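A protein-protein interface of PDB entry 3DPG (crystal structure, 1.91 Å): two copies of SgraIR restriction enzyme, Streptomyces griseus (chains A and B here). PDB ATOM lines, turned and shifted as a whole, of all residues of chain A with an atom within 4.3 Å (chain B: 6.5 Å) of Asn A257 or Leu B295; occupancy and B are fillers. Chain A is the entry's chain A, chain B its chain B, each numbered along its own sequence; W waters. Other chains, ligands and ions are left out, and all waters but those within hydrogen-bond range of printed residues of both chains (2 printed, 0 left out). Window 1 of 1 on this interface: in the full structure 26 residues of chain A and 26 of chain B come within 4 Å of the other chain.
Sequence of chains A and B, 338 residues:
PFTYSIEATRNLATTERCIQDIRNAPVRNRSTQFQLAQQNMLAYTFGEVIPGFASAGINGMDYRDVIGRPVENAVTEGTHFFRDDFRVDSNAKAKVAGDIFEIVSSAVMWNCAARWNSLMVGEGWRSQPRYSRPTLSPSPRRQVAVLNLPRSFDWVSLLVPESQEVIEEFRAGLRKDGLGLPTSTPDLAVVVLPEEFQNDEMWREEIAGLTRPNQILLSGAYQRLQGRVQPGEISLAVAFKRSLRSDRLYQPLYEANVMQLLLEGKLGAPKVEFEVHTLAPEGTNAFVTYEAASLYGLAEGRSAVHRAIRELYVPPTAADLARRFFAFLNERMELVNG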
ATOM      1  N   LEU A 181     -25.086  34.678  14.373  1.00  0.00           N
ATOM      2  CA  LEU A 181     -26.049  34.376  13.327  1.00  0.00           C
ATOM      3  C   LEU A 181     -27.154  35.421  13.334  1.00  0.00           C
ATOM      4  O   LEU A 181     -28.293  35.121  13.695  1.00  0.00           O
ATOM      5  CB  LEU A 181     -26.646  32.974  13.492  1.00  0.00           C
ATOM      6  CG  LEU A 181     -27.418  32.449  12.276  1.00  0.00           C
ATOM      7  CD1 LEU A 181     -26.489  32.181  11.096  1.00  0.00           C
ATOM      8  CD2 LEU A 181     -28.209  31.191  12.627  1.00  0.00           C
ATOM      9  N   LEU A 253     -32.535  35.603  -0.541  1.00  0.00           N
ATOM     10  CA  LEU A 253     -32.006  34.238  -0.608  1.00  0.00           C
ATOM     11  C   LEU A 253     -31.258  33.883   0.674  1.00  0.00           C
ATOM     12  O   LEU A 253     -31.427  32.789   1.221  1.00  0.00           O
ATOM     13  CB  LEU A 253     -31.107  34.058  -1.833  1.00  0.00           C
ATOM     14  CG  LEU A 253     -30.535  32.654  -2.058  1.00  0.00           C
ATOM     15  CD1 LEU A 253     -31.616  31.576  -1.989  1.00  0.00           C
ATOM     16  CD2 LEU A 253     -29.810  32.626  -3.401  1.00  0.00           C
ATOM     17  N   TYR A 254     -30.456  34.819   1.174  1.00  0.00           N
ATOM     18  CA  TYR A 254     -29.754  34.584   2.430  1.00  0.00           C
ATOM     19  C   TYR A 254     -30.687  34.568   3.644  1.00  0.00           C
ATOM     20  O   TYR A 254     -30.585  33.687   4.501  1.00  0.00           O
ATOM     21  CB  TYR A 254     -28.611  35.584   2.652  1.00  0.00           C
ATOM     22  CG  TYR A 254     -27.849  35.258   3.912  1.00  0.00           C
ATOM     23  CD1 TYR A 254     -26.894  34.243   3.923  1.00  0.00           C
ATOM     24  CD2 TYR A 254     -28.103  35.937   5.089  1.00  0.00           C
ATOM     25  CE1 TYR A 254     -26.218  33.923   5.080  1.00  0.00           C
ATOM     26  CE2 TYR A 254     -27.439  35.629   6.242  1.00  0.00           C
ATOM     27  CZ  TYR A 254     -26.493  34.620   6.233  1.00  0.00           C
ATOM     28  OH  TYR A 254     -25.829  34.315   7.385  1.00  0.00           O
ATOM     29  N   GLU A 255     -31.588  35.544   3.737  1.00  0.00           N
ATOM     30  CA  GLU A 255     -32.495  35.572   4.874  1.00  0.00           C
ATOM     31  C   GLU A 255     -33.395  34.331   4.905  1.00  0.00           C
ATOM     32  O   GLU A 255     -33.673  33.787   5.978  1.00  0.00           O
ATOM     33  CB  GLU A 255     -33.338  36.854   4.893  1.00  0.00           C
ATOM     34  CG  GLU A 255     -33.943  37.152   6.264  1.00  0.00           C
ATOM     35  CD  GLU A 255     -32.911  37.126   7.395  1.00  0.00           C
ATOM     36  OE1 GLU A 255     -33.247  36.632   8.494  1.00  0.00           O
ATOM     37  OE2 GLU A 255     -31.769  37.594   7.193  1.00  0.00           O
ATOM     38  N   ALA A 256     -33.846  33.886   3.736  1.00  0.00           N
ATOM     39  CA  ALA A 256     -34.667  32.684   3.662  1.00  0.00           C
ATOM     40  C   ALA A 256     -33.886  31.522   4.265  1.00  0.00           C
ATOM     41  O   ALA A 256     -34.424  30.727   5.032  1.00  0.00           O
ATOM     42  CB  ALA A 256     -35.039  32.369   2.213  1.00  0.00           C
ATOM     43  N   ASN A 257     -32.608  31.436   3.908  1.00  0.00           N
ATOM     44  CA  ASN A 257     -31.738  30.389   4.432  1.00  0.00           C
ATOM     45  C   ASN A 257     -31.622  30.417   5.951  1.00  0.00           C
ATOM     46  O   ASN A 257     -31.777  29.385   6.602  1.00  0.00           O
ATOM     47  CB  ASN A 257     -30.368  30.427   3.752  1.00  0.00           C
ATOM     48  CG  ASN A 257     -30.310  29.524   2.536  1.00  0.00           C
ATOM     49  OD1 ASN A 257     -30.240  28.299   2.669  1.00  0.00           O
ATOM     50  ND2 ASN A 257     -30.350  30.118   1.342  1.00  0.00           N
ATOM     51  N   VAL A 258     -31.413  31.603   6.515  1.00  0.00           N
ATOM     52  CA  VAL A 258     -31.335  31.757   7.965  1.00  0.00           C
ATOM     53  C   VAL A 258     -32.663  31.409   8.662  1.00  0.00           C
ATOM     54  O   VAL A 258     -32.672  30.706   9.674  1.00  0.00           O
ATOM     55  CB  VAL A 258     -30.876  33.179   8.366  1.00  0.00           C
ATOM     56  CG1 VAL A 258     -30.997  33.370   9.868  1.00  0.00           C
ATOM     57  CG2 VAL A 258     -29.422  33.440   7.895  1.00  0.00           C
ATOM     58  N   MET A 259     -33.779  31.899   8.124  1.00  0.00           N
ATOM     59  CA  MET A 259     -35.097  31.596   8.684  1.00  0.00           C
ATOM     60  C   MET A 259     -35.329  30.090   8.737  1.00  0.00           C
ATOM     61  O   MET A 259     -35.845  29.570   9.717  1.00  0.00           O
ATOM     62  CB  MET A 259     -36.215  32.267   7.872  1.00  0.00           C
ATOM     63  CG  MET A 259     -36.229  33.785   7.953  1.00  0.00           C
ATOM     64  SD  MET A 259     -37.686  34.544   7.155  1.00  0.00           S
ATOM     65  CE  MET A 259     -38.998  33.946   8.209  1.00  0.00           C
ATOM     66  N   GLN A 260     -34.943  29.405   7.667  1.00  0.00           N
ATOM     67  CA  GLN A 260     -35.117  27.968   7.556  1.00  0.00           C
ATOM     68  C   GLN A 260     -34.212  27.205   8.527  1.00  0.00           C
ATOM     69  O   GLN A 260     -34.646  26.234   9.148  1.00  0.00           O
ATOM     70  CB  GLN A 260     -34.912  27.525   6.105  1.00  0.00           C
ATOM     71  CG  GLN A 260     -36.101  27.901   5.236  1.00  0.00           C
ATOM     72  CD  GLN A 260     -35.779  28.096   3.770  1.00  0.00           C
ATOM     73  OE1 GLN A 260     -34.627  27.971   3.332  1.00  0.00           O
ATOM     74  NE2 GLN A 260     -36.807  28.428   2.999  1.00  0.00           N
ATOM     75  N   LEU A 261     -32.969  27.654   8.668  1.00  0.00           N
ATOM     76  CA  LEU A 261     -32.045  27.049   9.623  1.00  0.00           C
ATOM     77  C   LEU A 261     -32.610  27.153  11.032  1.00  0.00           C
ATOM     78  O   LEU A 261     -32.668  26.168  11.759  1.00  0.00           O
ATOM     79  CB  LEU A 261     -30.672  27.732   9.566  1.00  0.00           C
ATOM     80  CG  LEU A 261     -29.525  27.095  10.366  1.00  0.00           C
ATOM     81  CD1 LEU A 261     -28.171  27.469   9.757  1.00  0.00           C
ATOM     82  CD2 LEU A 261     -29.579  27.466  11.852  1.00  0.00           C
ATOM     83  N   SER A 294     -32.331  25.126  -0.117  1.00  0.00           N
ATOM     84  CA  SER A 294     -31.990  25.665   1.188  1.00  0.00           C
ATOM     85  C   SER A 294     -30.767  24.899   1.665  1.00  0.00           C
ATOM     86  O   SER A 294     -30.705  23.681   1.506  1.00  0.00           O
ATOM     87  CB  SER A 294     -33.148  25.481   2.166  1.00  0.00           C
ATOM     88  OG  SER A 294     -32.845  26.032   3.441  1.00  0.00           O
ATOM     89  N   LEU A 295     -29.797  25.604   2.242  1.00  0.00           N
ATOM     90  CA  LEU A 295     -28.498  25.000   2.528  1.00  0.00           C
ATOM     91  C   LEU A 295     -28.518  24.026   3.703  1.00  0.00           C
ATOM     92  O   LEU A 295     -27.930  22.953   3.623  1.00  0.00           O
ATOM     93  CB  LEU A 295     -27.439  26.078   2.778  1.00  0.00           C
ATOM     94  CG  LEU A 295     -27.202  27.108   1.674  1.00  0.00           C
ATOM     95  CD1 LEU A 295     -25.933  27.889   1.964  1.00  0.00           C
ATOM     96  CD2 LEU A 295     -27.111  26.447   0.310  1.00  0.00           C
ATOM     97  N   ALA A 308     -34.940  27.281  -1.095  1.00  0.00           N
ATOM     98  CA  ALA A 308     -34.896  28.360  -0.118  1.00  0.00           C
ATOM     99  C   ALA A 308     -36.033  29.329  -0.430  1.00  0.00           C
ATOM    100  O   ALA A 308     -36.824  29.675   0.444  1.00  0.00           O
ATOM    101  CB  ALA A 308     -33.555  29.080  -0.187  1.00  0.00           C
ATOM    102  N   TYR B 254     -23.620  35.082   0.763  1.00  0.00           N
ATOM    103  CA  TYR B 254     -24.244  33.893   0.184  1.00  0.00           C
ATOM    104  C   TYR B 254     -23.257  33.058  -0.625  1.00  0.00           C
ATOM    105  O   TYR B 254     -23.194  31.841  -0.461  1.00  0.00           O
ATOM    106  CB  TYR B 254     -25.458  34.217  -0.690  1.00  0.00           C
ATOM    107  CG  TYR B 254     -26.080  32.939  -1.219  1.00  0.00           C
ATOM    108  CD1 TYR B 254     -26.841  32.130  -0.387  1.00  0.00           C
ATOM    109  CD2 TYR B 254     -25.846  32.509  -2.522  1.00  0.00           C
ATOM    110  CE1 TYR B 254     -27.385  30.941  -0.842  1.00  0.00           C
ATOM    111  CE2 TYR B 254     -26.380  31.320  -2.989  1.00  0.00           C
ATOM    112  CZ  TYR B 254     -27.160  30.545  -2.143  1.00  0.00           C
ATOM    113  OH  TYR B 254     -27.699  29.353  -2.582  1.00  0.00           O
ATOM    114  N   ASN B 257     -20.856  30.999   1.481  1.00  0.00           N
ATOM    115  CA  ASN B 257     -21.536  29.811   1.997  1.00  0.00           C
ATOM    116  C   ASN B 257     -21.571  28.687   0.976  1.00  0.00           C
ATOM    117  O   ASN B 257     -21.244  27.542   1.296  1.00  0.00           O
ATOM    118  CB  ASN B 257     -22.955  30.154   2.465  1.00  0.00           C
ATOM    119  CG  ASN B 257     -22.986  30.646   3.892  1.00  0.00           C
ATOM    120  OD1 ASN B 257     -22.851  29.863   4.832  1.00  0.00           O
ATOM    121  ND2 ASN B 257     -23.150  31.952   4.067  1.00  0.00           N
ATOM    122  N   GLN B 260     -18.159  27.258   0.394  1.00  0.00           N
ATOM    123  CA  GLN B 260     -17.770  26.419   1.512  1.00  0.00           C
ATOM    124  C   GLN B 260     -18.460  25.060   1.442  1.00  0.00           C
ATOM    125  O   GLN B 260     -17.844  24.023   1.709  1.00  0.00           O
ATOM    126  CB  GLN B 260     -18.046  27.123   2.837  1.00  0.00           C
ATOM    127  CG  GLN B 260     -17.089  28.286   3.105  1.00  0.00           C
ATOM    128  CD  GLN B 260     -17.412  29.034   4.387  1.00  0.00           C
ATOM    129  OE1 GLN B 260     -18.550  29.030   4.850  1.00  0.00           O
ATOM    130  NE2 GLN B 260     -16.407  29.694   4.958  1.00  0.00           N
ATOM    131  N   ALA B 292     -21.180  36.317  10.686  1.00  0.00           N
ATOM    132  CA  ALA B 292     -22.070  35.154  10.626  1.00  0.00           C
ATOM    133  C   ALA B 292     -21.327  33.837  10.415  1.00  0.00           C
ATOM    134  O   ALA B 292     -20.442  33.738   9.557  1.00  0.00           O
ATOM    135  CB  ALA B 292     -23.122  35.334   9.542  1.00  0.00           C
ATOM    136  N   ALA B 293     -21.707  32.828  11.197  1.00  0.00           N
ATOM    137  CA  ALA B 293     -21.192  31.481  11.011  1.00  0.00           C
ATOM    138  C   ALA B 293     -21.608  30.962   9.652  1.00  0.00           C
ATOM    139  O   ALA B 293     -22.682  31.303   9.151  1.00  0.00           O
ATOM    140  CB  ALA B 293     -21.710  30.556  12.100  1.00  0.00           C
ATOM    141  N   SER B 294     -20.743  30.145   9.058  1.00  0.00           N
ATOM    142  CA  SER B 294     -21.060  29.410   7.840  1.00  0.00           C
ATOM    143  C   SER B 294     -22.330  28.590   8.057  1.00  0.00           C
ATOM    144  O   SER B 294     -22.423  27.829   9.021  1.00  0.00           O
ATOM    145  CB  SER B 294     -19.906  28.477   7.479  1.00  0.00           C
ATOM    146  OG  SER B 294     -20.200  27.689   6.334  1.00  0.00           O
ATOM    147  N   LEU B 295     -23.309  28.757   7.170  1.00  0.00           N
ATOM    148  CA  LEU B 295     -24.560  28.007   7.262  1.00  0.00           C
ATOM    149  C   LEU B 295     -24.307  26.516   7.097  1.00  0.00           C
ATOM    150  O   LEU B 295     -24.817  25.704   7.871  1.00  0.00           O
ATOM    151  CB  LEU B 295     -25.565  28.490   6.214  1.00  0.00           C
ATOM    152  CG  LEU B 295     -25.928  29.973   6.327  1.00  0.00           C
ATOM    153  CD1 LEU B 295     -27.227  30.266   5.578  1.00  0.00           C
ATOM    154  CD2 LEU B 295     -26.056  30.371   7.787  1.00  0.00           C
ATOM    155  N   TYR B 296     -23.509  26.135   6.106  1.00  0.00           N
ATOM    156  CA  TYR B 296     -23.245  24.714   5.906  1.00  0.00           C
ATOM    157  C   TYR B 296     -22.218  24.181   6.907  1.00  0.00           C
ATOM    158  O   TYR B 296     -22.113  22.971   7.109  1.00  0.00           O
ATOM    159  CB  TYR B 296     -22.838  24.402   4.467  1.00  0.00           C
ATOM    160  CG  TYR B 296     -22.990  22.938   4.108  1.00  0.00           C
ATOM    161  CD1 TYR B 296     -24.250  22.364   3.962  1.00  0.00           C
ATOM    162  CD2 TYR B 296     -21.876  22.128   3.919  1.00  0.00           C
ATOM    163  CE1 TYR B 296     -24.392  21.028   3.634  1.00  0.00           C
ATOM    164  CE2 TYR B 296     -22.012  20.791   3.593  1.00  0.00           C
ATOM    165  CZ  TYR B 296     -23.271  20.247   3.453  1.00  0.00           C
ATOM    166  OH  TYR B 296     -23.402  18.920   3.125  1.00  0.00           O
ATOM    167  N   GLY B 297     -21.464  25.086   7.530  1.00  0.00           N
ATOM    168  CA  GLY B 297     -20.650  24.718   8.673  1.00  0.00           C
ATOM    169  C   GLY B 297     -21.541  24.348   9.849  1.00  0.00           C
ATOM    170  O   GLY B 297     -21.297  23.355  10.542  1.00  0.00           O
ATOM    171  N   LEU B 298     -22.580  25.148  10.078  1.00  0.00           N
ATOM    172  CA  LEU B 298     -23.549  24.847  11.129  1.00  0.00           C
ATOM    173  C   LEU B 298     -24.306  23.574  10.783  1.00  0.00           C
ATOM    174  O   LEU B 298     -24.574  22.736  11.649  1.00  0.00           O
ATOM    175  CB  LEU B 298     -24.532  26.005  11.317  1.00  0.00           C
ATOM    176  CG  LEU B 298     -24.004  27.254  12.027  1.00  0.00           C
ATOM    177  CD1 LEU B 298     -25.045  28.372  11.979  1.00  0.00           C
ATOM    178  CD2 LEU B 298     -23.616  26.930  13.468  1.00  0.00           C
ATOM    179  N   ALA B 299     -24.640  23.431   9.504  1.00  0.00           N
ATOM    180  CA  ALA B 299     -25.376  22.269   9.030  1.00  0.00           C
ATOM    181  C   ALA B 299     -24.611  20.981   9.333  1.00  0.00           C
ATOM    182  O   ALA B 299     -25.187  19.995   9.789  1.00  0.00           O
ATOM    183  CB  ALA B 299     -25.648  22.388   7.541  1.00  0.00           C
ATOM    184  N   GLU B 300     -23.307  20.992   9.078  1.00  0.00           N
ATOM    185  CA  GLU B 300     -22.490  19.800   9.286  1.00  0.00           C
ATOM    186  C   GLU B 300     -22.199  19.546  10.758  1.00  0.00           C
ATOM    187  O   GLU B 300     -22.130  18.394  11.191  1.00  0.00           O
ATOM    188  CB  GLU B 300     -21.194  19.880   8.482  1.00  0.00           C
ATOM    189  CG  GLU B 300     -21.411  19.707   6.994  1.00  0.00           C
ATOM    190  CD  GLU B 300     -22.130  18.417   6.659  1.00  0.00           C
ATOM    191  OE1 GLU B 300     -22.297  17.571   7.565  1.00  0.00           O
ATOM    192  OE2 GLU B 300     -22.521  18.242   5.487  1.00  0.00           O
ATOM    193  N   HIS B 306     -16.539  27.823  11.216  1.00  0.00           N
ATOM    194  CA  HIS B 306     -15.941  29.122  10.918  1.00  0.00           C
ATOM    195  C   HIS B 306     -16.894  30.060  10.179  1.00  0.00           C
ATOM    196  O   HIS B 306     -17.910  29.630   9.632  1.00  0.00           O
ATOM    197  CB  HIS B 306     -14.624  28.975  10.154  1.00  0.00           C
ATOM    198  CG  HIS B 306     -14.705  28.094   8.944  1.00  0.00           C
ATOM    199  ND1 HIS B 306     -15.160  28.543   7.724  1.00  0.00           N
ATOM    200  CD2 HIS B 306     -14.350  26.800   8.760  1.00  0.00           C
ATOM    201  CE1 HIS B 306     -15.102  27.559   6.844  1.00  0.00           C
ATOM    202  NE2 HIS B 306     -14.611  26.491   7.447  1.00  0.00           N
ATOM    203  N   ALA B 308     -18.515  32.531   7.387  1.00  0.00           N
ATOM    204  CA  ALA B 308     -18.578  32.474   5.934  1.00  0.00           C
ATOM    205  C   ALA B 308     -17.592  33.490   5.349  1.00  0.00           C
ATOM    206  O   ALA B 308     -16.832  33.177   4.430  1.00  0.00           O
ATOM    207  CB  ALA B 308     -20.008  32.761   5.448  1.00  0.00           C
HETATM  208  O   HOH W   1     -29.964  28.483  -0.920  1.00  0.00           O
HETATM  209  O   HOH W   2     -23.467  32.749   6.962  1.00  0.00           O
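Among the printed residues, pairs that only touch across the chains: Leu A181 with Leu B295 (3.8 Å), Leu A253 with Tyr B254 (3.6 Å), Tyr A254 with Asn B257 (3.8 Å), Tyr A254 with Ala B292 (3.6 Å), Tyr A254 with Leu B295 (3.8 Å), Asn A257 with Tyr B254 (3.8 Å), Asn A257 with Leu B295 (3.6 Å), Leu A261 with Leu B298 (3.9 Å), Leu A295 with Asn B257 (3.8 Å) and Leu A295 with Tyr B296 (3.7 Å).
The side-chain amide oxygen (OD1) of Asn A257 is in hydrogen-bond range of the backbone NH (N) of Leu A295, 2.8 Å away.
The backbone carbonyl oxygen (O) of Leu A253 is in hydrogen-bond range of the side-chain amide nitrogen (ND2) of Asn A257 (2.9 Å).
N of Leu B295 lies within hydrogen-bond range of OD1 of Asn B257 (2.6 Å).
The side-chain hydroxyl (OH) of Tyr B296 is in hydrogen-bond range of the side-chain carboxylate (OE2) of Glu B300 (2.6 Å).
The backbone carbonyl oxygen of Ala B292 is in hydrogen-bond range of the backbone NH of Ala B308 (3.1 Å).
Water W2 lies within hydrogen-bond range of O of Ala B293 (2.7 Å), OH of Tyr A254 (2.9 Å) and ND2 of Asn B257 (3.0 Å).
Water W1 bridges the side-chain amide nitrogen (ND2) of Asn A257 (2.8 Å) and the side-chain hydroxyl (OH) of Tyr B254 (2.9 Å).
Tyr A254 touches Asn B257, and with the chains exchanged Asn A257 touches Tyr B254.
Tyr A254 touches Leu B295, but with the chains exchanged Leu A295 does not touch Tyr B254 (4.1 Å).
Asn A257 touches Leu B295, and with the chains exchanged Leu A295 touches Asn B257.
6 positions are printed for both chains.
Printed residues of chain A that touch a printed residue of chain B: Leu A181, Leu A253, Tyr A254, Asn A257, Leu A261 and Leu A295.
Hydrophobic or aromatic side chains of chain A that line the printed part of chain B: Leu A181, Leu A253, Tyr A254, Leu A261 and Leu A295.
Of chain B, only Tyr B254 and Leu B295 come within 4 Å of Asn A257.
Leu B295 touches just these residues of chain A: Leu A181 (3.8 Å), Tyr A254 (3.8 Å) and Asn A257 (3.6 Å).
Of the printed residues of chain B, Tyr A254 touches Asn B257 (3.8 Å), Ala B292 (3.6 Å) and Leu B295 (3.8 Å).
Of the printed residues of chain B, Leu A253 touches Tyr B254.
Ala A308 touches none of the printed residues of chain B.
Glu A255 touches none of the printed residues of chain B.
The nearest printed residue of chain B that does not touch Asn A257 is Asn B257 (7.4 Å).
The nearest printed residue of chain A that does not touch Leu B298 is Leu A181 (4.2 Å).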
